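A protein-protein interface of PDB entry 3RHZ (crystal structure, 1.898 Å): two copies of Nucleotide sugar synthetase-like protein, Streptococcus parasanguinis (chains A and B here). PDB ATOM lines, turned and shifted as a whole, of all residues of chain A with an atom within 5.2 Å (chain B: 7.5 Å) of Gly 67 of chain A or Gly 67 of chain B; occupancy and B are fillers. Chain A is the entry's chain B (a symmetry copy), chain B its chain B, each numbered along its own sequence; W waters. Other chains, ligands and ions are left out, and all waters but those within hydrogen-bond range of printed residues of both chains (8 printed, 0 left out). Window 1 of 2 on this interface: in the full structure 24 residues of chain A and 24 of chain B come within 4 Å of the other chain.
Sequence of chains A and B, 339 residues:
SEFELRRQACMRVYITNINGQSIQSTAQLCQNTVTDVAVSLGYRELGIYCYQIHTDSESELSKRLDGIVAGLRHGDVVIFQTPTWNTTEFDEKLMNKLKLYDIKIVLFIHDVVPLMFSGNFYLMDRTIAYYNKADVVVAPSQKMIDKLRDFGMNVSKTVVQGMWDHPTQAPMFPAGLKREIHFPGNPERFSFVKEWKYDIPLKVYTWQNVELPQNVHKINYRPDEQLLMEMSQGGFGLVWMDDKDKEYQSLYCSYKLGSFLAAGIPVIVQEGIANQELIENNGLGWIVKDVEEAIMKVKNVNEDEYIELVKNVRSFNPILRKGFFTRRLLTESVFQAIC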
ATOM      1  N   GLY A  47       2.065  28.951 -10.081  1.00  0.00           N
ATOM      2  CA  GLY A  47       2.451  30.059 -10.928  1.00  0.00           C
ATOM      3  C   GLY A  47       1.617  30.121 -12.197  1.00  0.00           C
ATOM      4  O   GLY A  47       1.275  29.092 -12.789  1.00  0.00           O
ATOM      5  N   LYS A  63      -4.133  21.403 -21.303  1.00  0.00           N
ATOM      6  CA  LYS A  63      -2.906  20.788 -20.799  1.00  0.00           C
ATOM      7  C   LYS A  63      -1.953  21.792 -20.155  1.00  0.00           C
ATOM      8  O   LYS A  63      -1.232  21.458 -19.223  1.00  0.00           O
ATOM      9  CB  LYS A  63      -2.227  20.000 -21.914  1.00  0.00           C
ATOM     10  CG  LYS A  63      -3.111  18.878 -22.380  1.00  0.00           C
ATOM     11  CD  LYS A  63      -2.439  18.027 -23.420  1.00  0.00           C
ATOM     12  CE  LYS A  63      -3.341  16.861 -23.783  1.00  0.00           C
ATOM     13  NZ  LYS A  63      -2.581  15.858 -24.550  1.00  0.00           N
ATOM     14  N   ARG A  64      -1.942  23.024 -20.654  1.00  0.00           N
ATOM     15  CA  ARG A  64      -1.227  24.094 -19.948  1.00  0.00           C
ATOM     16  C   ARG A  64      -1.764  24.227 -18.528  1.00  0.00           C
ATOM     17  O   ARG A  64      -1.001  24.354 -17.559  1.00  0.00           O
ATOM     18  CB  ARG A  64      -1.390  25.431 -20.700  1.00  0.00           C
ATOM     19  CG  ARG A  64      -0.612  26.578 -20.074  1.00  0.00           C
ATOM     20  CD  ARG A  64      -1.016  27.935 -20.647  1.00  0.00           C
ATOM     21  NE  ARG A  64      -0.810  28.029 -22.084  1.00  0.00           N
ATOM     22  CZ  ARG A  64       0.334  28.391 -22.657  1.00  0.00           C
ATOM     23  NH1 ARG A  64       1.379  28.711 -21.903  1.00  0.00           N
ATOM     24  NH2 ARG A  64       0.418  28.465 -23.980  1.00  0.00           N
ATOM     25  N   LEU A  65      -3.085  24.209 -18.390  1.00  0.00           N
ATOM     26  CA  LEU A  65      -3.700  24.271 -17.060  1.00  0.00           C
ATOM     27  C   LEU A  65      -3.342  23.042 -16.218  1.00  0.00           C
ATOM     28  O   LEU A  65      -3.117  23.145 -15.005  1.00  0.00           O
ATOM     29  CB  LEU A  65      -5.217  24.398 -17.187  1.00  0.00           C
ATOM     30  CG  LEU A  65      -5.744  25.763 -17.634  1.00  0.00           C
ATOM     31  CD1 LEU A  65      -7.197  25.635 -18.028  1.00  0.00           C
ATOM     32  CD2 LEU A  65      -5.572  26.796 -16.522  1.00  0.00           C
ATOM     33  N   ASP A  66      -3.294  21.878 -16.859  1.00  0.00           N
ATOM     34  CA  ASP A  66      -2.859  20.662 -16.171  1.00  0.00           C
ATOM     35  C   ASP A  66      -1.425  20.793 -15.652  1.00  0.00           C
ATOM     36  O   ASP A  66      -1.075  20.263 -14.586  1.00  0.00           O
ATOM     37  CB  ASP A  66      -2.954  19.457 -17.108  1.00  0.00           C
ATOM     38  CG  ASP A  66      -4.385  18.991 -17.327  1.00  0.00           C
ATOM     39  OD1 ASP A  66      -5.280  19.409 -16.566  1.00  0.00           O
ATOM     40  OD2 ASP A  66      -4.607  18.179 -18.253  1.00  0.00           O
ATOM     41  N   GLY A  67      -0.593  21.492 -16.412  1.00  0.00           N
ATOM     42  CA  GLY A  67       0.766  21.748 -15.989  1.00  0.00           C
ATOM     43  C   GLY A  67       0.789  22.644 -14.760  1.00  0.00           C
ATOM     44  O   GLY A  67       1.544  22.398 -13.823  1.00  0.00           O
ATOM     45  N   ILE A  68      -0.038  23.683 -14.765  1.00  0.00           N
ATOM     46  CA  ILE A  68      -0.134  24.594 -13.631  1.00  0.00           C
ATOM     47  C   ILE A  68      -0.585  23.869 -12.357  1.00  0.00           C
ATOM     48  O   ILE A  68      -0.002  24.054 -11.288  1.00  0.00           O
ATOM     49  CB  ILE A  68      -1.084  25.797 -13.948  1.00  0.00           C
ATOM     50  CG1 ILE A  68      -0.479  26.694 -15.032  1.00  0.00           C
ATOM     51  CG2 ILE A  68      -1.377  26.617 -12.703  1.00  0.00           C
ATOM     52  CD1 ILE A  68      -1.487  27.687 -15.648  1.00  0.00           C
ATOM     53  N   VAL A  69      -1.597  23.011 -12.480  1.00  0.00           N
ATOM     54  CA  VAL A  69      -2.188  22.355 -11.307  1.00  0.00           C
ATOM     55  C   VAL A  69      -1.600  20.965 -11.018  1.00  0.00           C
ATOM     56  O   VAL A  69      -2.149  20.208 -10.218  1.00  0.00           O
ATOM     57  CB  VAL A  69      -3.732  22.251 -11.430  1.00  0.00           C
ATOM     58  CG1 VAL A  69      -4.368  23.638 -11.493  1.00  0.00           C
ATOM     59  CG2 VAL A  69      -4.132  21.408 -12.657  1.00  0.00           C
ATOM     60  N   ALA A  70      -0.487  20.635 -11.666  1.00  0.00           N
ATOM     61  CA  ALA A  70       0.072  19.285 -11.595  1.00  0.00           C
ATOM     62  C   ALA A  70       0.331  18.784 -10.158  1.00  0.00           C
ATOM     63  O   ALA A  70       0.193  17.591  -9.880  1.00  0.00           O
ATOM     64  CB  ALA A  70       1.352  19.206 -12.422  1.00  0.00           C
ATOM     65  N   LEU B  46       7.821  23.102  -8.116  1.00  0.00           N
ATOM     66  CA  LEU B  46       7.360  22.986  -9.496  1.00  0.00           C
ATOM     67  C   LEU B  46       6.771  21.591  -9.638  1.00  0.00           C
ATOM     68  O   LEU B  46       7.499  20.638  -9.844  1.00  0.00           O
ATOM     69  CB  LEU B  46       8.516  23.130 -10.482  1.00  0.00           C
ATOM     70  CG  LEU B  46       9.247  24.466 -10.510  1.00  0.00           C
ATOM     71  CD1 LEU B  46      10.444  24.382 -11.444  1.00  0.00           C
ATOM     72  CD2 LEU B  46       8.275  25.572 -10.946  1.00  0.00           C
ATOM     73  N   GLY B  47       5.458  21.480  -9.513  1.00  0.00           N
ATOM     74  CA  GLY B  47       4.806  20.188  -9.500  1.00  0.00           C
ATOM     75  C   GLY B  47       4.798  19.544 -10.876  1.00  0.00           C
ATOM     76  O   GLY B  47       4.626  20.216 -11.897  1.00  0.00           O
ATOM     77  N   ILE B  48       4.983  18.233 -10.899  1.00  0.00           N
ATOM     78  CA  ILE B  48       4.992  17.475 -12.149  1.00  0.00           C
ATOM     79  C   ILE B  48       4.077  16.270 -12.031  1.00  0.00           C
ATOM     80  O   ILE B  48       4.249  15.455 -11.133  1.00  0.00           O
ATOM     81  CB  ILE B  48       6.407  17.001 -12.510  1.00  0.00           C
ATOM     82  CG1 ILE B  48       7.330  18.212 -12.695  1.00  0.00           C
ATOM     83  CG2 ILE B  48       6.363  16.091 -13.763  1.00  0.00           C
ATOM     84  CD1 ILE B  48       8.747  17.869 -13.030  1.00  0.00           C
ATOM     85  N   TYR B  49       3.090  16.154 -12.913  1.00  0.00           N
ATOM     86  CA  TYR B  49       2.206  14.998 -12.821  1.00  0.00           C
ATOM     87  C   TYR B  49       2.733  13.860 -13.688  1.00  0.00           C
ATOM     88  O   TYR B  49       3.218  14.093 -14.795  1.00  0.00           O
ATOM     89  CB  TYR B  49       0.776  15.364 -13.205  1.00  0.00           C
ATOM     90  CG  TYR B  49      -0.236  14.406 -12.634  1.00  0.00           C
ATOM     91  CD1 TYR B  49      -0.737  14.587 -11.356  1.00  0.00           C
ATOM     92  CD2 TYR B  49      -0.688  13.322 -13.370  1.00  0.00           C
ATOM     93  CE1 TYR B  49      -1.660  13.719 -10.822  1.00  0.00           C
ATOM     94  CE2 TYR B  49      -1.620  12.448 -12.848  1.00  0.00           C
ATOM     95  CZ  TYR B  49      -2.098  12.650 -11.570  1.00  0.00           C
ATOM     96  OH  TYR B  49      -3.023  11.789 -11.028  1.00  0.00           O
ATOM     97  N   LEU B  61       2.725  19.240 -25.351  1.00  0.00           N
ATOM     98  CA  LEU B  61       3.749  18.971 -24.333  1.00  0.00           C
ATOM     99  C   LEU B  61       4.520  20.255 -24.019  1.00  0.00           C
ATOM    100  O   LEU B  61       4.874  20.523 -22.881  1.00  0.00           O
ATOM    101  CB  LEU B  61       4.711  17.879 -24.798  1.00  0.00           C
ATOM    102  CG  LEU B  61       5.929  17.667 -23.895  1.00  0.00           C
ATOM    103  CD1 LEU B  61       5.502  17.263 -22.483  1.00  0.00           C
ATOM    104  CD2 LEU B  61       6.848  16.628 -24.514  1.00  0.00           C
ATOM    105  N   SER B  62       4.780  21.051 -25.049  1.00  0.00           N
ATOM    106  CA  SER B  62       5.507  22.300 -24.864  1.00  0.00           C
ATOM    107  C   SER B  62       4.739  23.228 -23.932  1.00  0.00           C
ATOM    108  O   SER B  62       5.320  23.859 -23.052  1.00  0.00           O
ATOM    109  CB  SER B  62       5.714  22.996 -26.219  1.00  0.00           C
ATOM    110  OG  SER B  62       6.572  24.121 -26.083  1.00  0.00           O
ATOM    111  N   LYS B  63       3.428  23.326 -24.135  1.00  0.00           N
ATOM    112  CA  LYS B  63       2.621  24.234 -23.319  1.00  0.00           C
ATOM    113  C   LYS B  63       2.315  23.678 -21.930  1.00  0.00           C
ATOM    114  O   LYS B  63       2.196  24.429 -20.970  1.00  0.00           O
ATOM    115  CB  LYS B  63       1.348  24.609 -24.069  1.00  0.00           C
ATOM    116  CG  LYS B  63       1.681  25.350 -25.333  1.00  0.00           C
ATOM    117  CD  LYS B  63       0.447  25.813 -26.057  1.00  0.00           C
ATOM    118  CE  LYS B  63       0.847  26.630 -27.272  1.00  0.00           C
ATOM    119  NZ  LYS B  63      -0.326  27.346 -27.803  1.00  0.00           N
ATOM    120  N   ARG B  64       2.180  22.360 -21.820  1.00  0.00           N
ATOM    121  CA  ARG B  64       2.112  21.738 -20.491  1.00  0.00           C
ATOM    122  C   ARG B  64       3.357  22.096 -19.688  1.00  0.00           C
ATOM    123  O   ARG B  64       3.281  22.445 -18.502  1.00  0.00           O
ATOM    124  CB  ARG B  64       1.994  20.207 -20.625  1.00  0.00           C
ATOM    125  CG  ARG B  64       1.840  19.491 -19.291  1.00  0.00           C
ATOM    126  CD  ARG B  64       2.021  17.980 -19.418  1.00  0.00           C
ATOM    127  NE  ARG B  64       1.067  17.368 -20.330  1.00  0.00           N
ATOM    128  CZ  ARG B  64      -0.148  16.957 -19.981  1.00  0.00           C
ATOM    129  NH1 ARG B  64      -0.553  17.081 -18.723  1.00  0.00           N
ATOM    130  NH2 ARG B  64      -0.940  16.391 -20.884  1.00  0.00           N
ATOM    131  N   LEU B  65       4.520  22.005 -20.325  1.00  0.00           N
ATOM    132  CA  LEU B  65       5.770  22.384 -19.659  1.00  0.00           C
ATOM    133  C   LEU B  65       5.791  23.875 -19.309  1.00  0.00           C
ATOM    134  O   LEU B  65       6.290  24.274 -18.249  1.00  0.00           O
ATOM    135  CB  LEU B  65       6.965  22.032 -20.544  1.00  0.00           C
ATOM    136  CG  LEU B  65       7.319  20.546 -20.642  1.00  0.00           C
ATOM    137  CD1 LEU B  65       8.282  20.336 -21.787  1.00  0.00           C
ATOM    138  CD2 LEU B  65       7.919  20.049 -19.329  1.00  0.00           C
ATOM    139  N   ASP B  66       5.255  24.701 -20.203  1.00  0.00           N
ATOM    140  CA  ASP B  66       5.129  26.130 -19.921  1.00  0.00           C
ATOM    141  C   ASP B  66       4.252  26.384 -18.693  1.00  0.00           C
ATOM    142  O   ASP B  66       4.488  27.321 -17.914  1.00  0.00           O
ATOM    143  CB  ASP B  66       4.541  26.862 -21.128  1.00  0.00           C
ATOM    144  CG  ASP B  66       5.542  27.030 -22.261  1.00  0.00           C
ATOM    145  OD1 ASP B  66       6.752  26.829 -22.034  1.00  0.00           O
ATOM    146  OD2 ASP B  66       5.113  27.390 -23.380  1.00  0.00           O
ATOM    147  N   GLY B  67       3.230  25.554 -18.526  1.00  0.00           N
ATOM    148  CA  GLY B  67       2.377  25.650 -17.362  1.00  0.00           C
ATOM    149  C   GLY B  67       3.148  25.303 -16.098  1.00  0.00           C
ATOM    150  O   GLY B  67       3.014  25.979 -15.081  1.00  0.00           O
ATOM    151  N   ILE B  68       3.953  24.248 -16.161  1.00  0.00           N
ATOM    152  CA  ILE B  68       4.771  23.838 -15.026  1.00  0.00           C
ATOM    153  C   ILE B  68       5.760  24.936 -14.612  1.00  0.00           C
ATOM    154  O   ILE B  68       5.894  25.247 -13.428  1.00  0.00           O
ATOM    155  CB  ILE B  68       5.525  22.499 -15.324  1.00  0.00           C
ATOM    156  CG1 ILE B  68       4.536  21.336 -15.447  1.00  0.00           C
ATOM    157  CG2 ILE B  68       6.555  22.191 -14.253  1.00  0.00           C
ATOM    158  CD1 ILE B  68       5.147  20.068 -16.079  1.00  0.00           C
ATOM    159  N   VAL B  69       6.420  25.550 -15.593  1.00  0.00           N
ATOM    160  CA  VAL B  69       7.476  26.528 -15.304  1.00  0.00           C
ATOM    161  C   VAL B  69       6.982  27.983 -15.299  1.00  0.00           C
ATOM    162  O   VAL B  69       7.785  28.915 -15.302  1.00  0.00           O
ATOM    163  CB  VAL B  69       8.668  26.387 -16.290  1.00  0.00           C
ATOM    164  CG1 VAL B  69       9.326  25.017 -16.157  1.00  0.00           C
ATOM    165  CG2 VAL B  69       8.214  26.639 -17.742  1.00  0.00           C
ATOM    166  N   ALA B  70       5.666  28.172 -15.288  1.00  0.00           N
ATOM    167  CA  ALA B  70       5.080  29.504 -15.443  1.00  0.00           C
ATOM    168  C   ALA B  70       5.601  30.545 -14.431  1.00  0.00           C
ATOM    169  O   ALA B  70       5.723  31.727 -14.759  1.00  0.00           O
ATOM    170  CB  ALA B  70       3.558  29.415 -15.377  1.00  0.00           C
ATOM    171  N   GLY B  71       5.901  30.109 -13.208  1.00  0.00           N
ATOM    172  CA  GLY B  71       6.307  31.026 -12.145  1.00  0.00           C
ATOM    173  C   GLY B  71       7.778  31.413 -12.185  1.00  0.00           C
ATOM    174  O   GLY B  71       8.215  32.285 -11.441  1.00  0.00           O
ATOM    175  N   LYS B  97      13.537  23.449 -21.507  1.00  0.00           N
ATOM    176  CA  LYS B  97      12.746  24.612 -21.099  1.00  0.00           C
ATOM    177  C   LYS B  97      13.515  25.435 -20.084  1.00  0.00           C
ATOM    178  O   LYS B  97      13.576  26.662 -20.176  1.00  0.00           O
ATOM    179  CB  LYS B  97      11.419  24.190 -20.458  1.00  0.00           C
ATOM    180  CG  LYS B  97      10.362  23.721 -21.429  1.00  0.00           C
ATOM    181  CD  LYS B  97       9.743  24.879 -22.198  1.00  0.00           C
ATOM    182  CE  LYS B  97       8.535  24.400 -22.986  1.00  0.00           C
ATOM    183  NZ  LYS B  97       7.977  25.439 -23.902  1.00  0.00           N
HETATM  184  O   HOH W   1       3.209  22.492 -11.678  1.00  0.00           O
HETATM  185  O   HOH W   2       3.612  29.631 -23.521  1.00  0.00           O
HETATM  186  O   HOH W   3       2.275  29.187 -19.054  1.00  0.00           O
HETATM  187  O   HOH W   4      -3.175  15.890 -18.329  1.00  0.00           O
HETATM  188  O   HOH W   5       0.346  17.848 -15.938  1.00  0.00           O
HETATM  189  O   HOH W   6       1.003  30.217 -26.517  1.00  0.00           O
HETATM  190  O   HOH W   7      -2.613  13.886 -21.763  1.00  0.00           O
HETATM  191  O   HOH W   8       2.842  26.920 -12.538  1.00  0.00           O
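Water W1 bridges O of Gly 47 of chain B and O of Gly 67 of chain A. Water W8 bridges the backbone carbonyl oxygen of Gly 47 of chain A (2.7 Å) and the backbone carbonyl oxygen of Gly 67 of chain B (2.7 Å). Water W2 lies within hydrogen-bond range of the side-chain carboxylate of Asp 66 of chain B (2.7 Å) and the guanidinium group of Arg 64 of chain A (2.9 Å). Water W5 bridges NH1 of Arg 64 of chain B (3.0 Å) and O of Asp 66 of chain A (3.1 Å). Water W7 bridges the guanidinium group (NH2) of Arg 64 of chain B (3.1 Å) and the side-chain amino group (NZ) of Lys 63 of chain A (3.4 Å). Water W6 lies within hydrogen-bond range of the guanidinium group (NH2) of Arg 64 of chain A and the side-chain amino group (NZ) of Lys 63 of chain B.
Printed residues of chain B that touch a printed residue of chain A: Gly 47, Tyr 49, Lys 63, Arg 64, Asp 66, Gly 67, Ile 68 and Ala 70. Hydrophobic or aromatic side chains of chain B that line the printed part of chain A: Tyr 49, Ile 68 and Ala 70.
Gly 47 of chain A touches Ala 70 of chain B (O to CB, 3.5 Å). Lys 63 of chain A touches Arg 64 of chain B. CB of Asp 66 of chain B touches NH1 of Arg 64 of chain A, at 3.7 Å. Arg 64 of chain A touches Gly 67 of chain B. NH1 of Arg 64 of chain B touches CB of Asp 66 of chain A, 3.7 Å away. Gly 67 of chain A touches Arg 64 of chain B (CA to O, 3.6 Å). O of Gly 67 of chain A touches CG1 of Ile 68 of chain B, 3.6 Å away. Gly 67 of chain B touches Ile 68 of chain A (O to CG1, 3.6 Å). Gly 47 of chain B touches Ala 70 of chain A (O to CB, 3.5 Å). Ala 70 of chain A touches Tyr 49 of chain B.
Gly 67 of chain A touches just these residues of chain B: Arg 64 (3.6 Å), Gly 67 (3.8 Å) and Ile 68 (3.6 Å). Printed residues of chain A within 4 Å of Gly 67 of chain B: Arg 64, Gly 67 and Ile 68. Printed residues of chain A within 4 Å of Ala 70 of chain B: Gly 47 (3.5 Å). Printed residues of chain A within 4 Å of Lys 63 of chain B: Arg 64 (3.4 Å). Printed residues of chain B within 4 Å of Ile 68 of chain A: Gly 67 (3.6 Å). Of the printed residues of chain A, Ile 68 of chain B touches Gly 67. Of the printed residues of chain A, Gly 47 of chain B touches Ala 70 (3.5 Å). The nearest residue of chain B that does not touch Gly 67 of chain A is Gly 47 of chain B (4.2 Å). The nearest residue of chain A that does not touch Gly 67 of chain B is Gly 47 of chain A (4.2 Å).
Gly 47 of chain A touches Ala 70 of chain B, and with the chains exchanged Ala 70 of chain A touches Gly 47 of chain B. Lys 63 of chain A touches Arg 64 of chain B, and with the chains exchanged Arg 64 of chain A touches Lys 63 of chain B. Arg 64 of chain A touches Asp 66 of chain B, and with the chains exchanged Asp 66 of chain A touches Arg 64 of chain B. Gly 67 of chain A touches its own counterpart, Gly 67 of chain B. Positions printed for both chains: 47, 63, 64, 65, 66, 67, 68, 69 and 70. Of the 12 pairs that touch across the chains among the printed residues, 11 have their exchanged pair printed and touching as well.
The side-chain amino group (NZ) of Lys 97 of chain B is in salt-bridge range of the side-chain carboxylate (OD1) of Asp 66 of chain B (2.6 Å).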
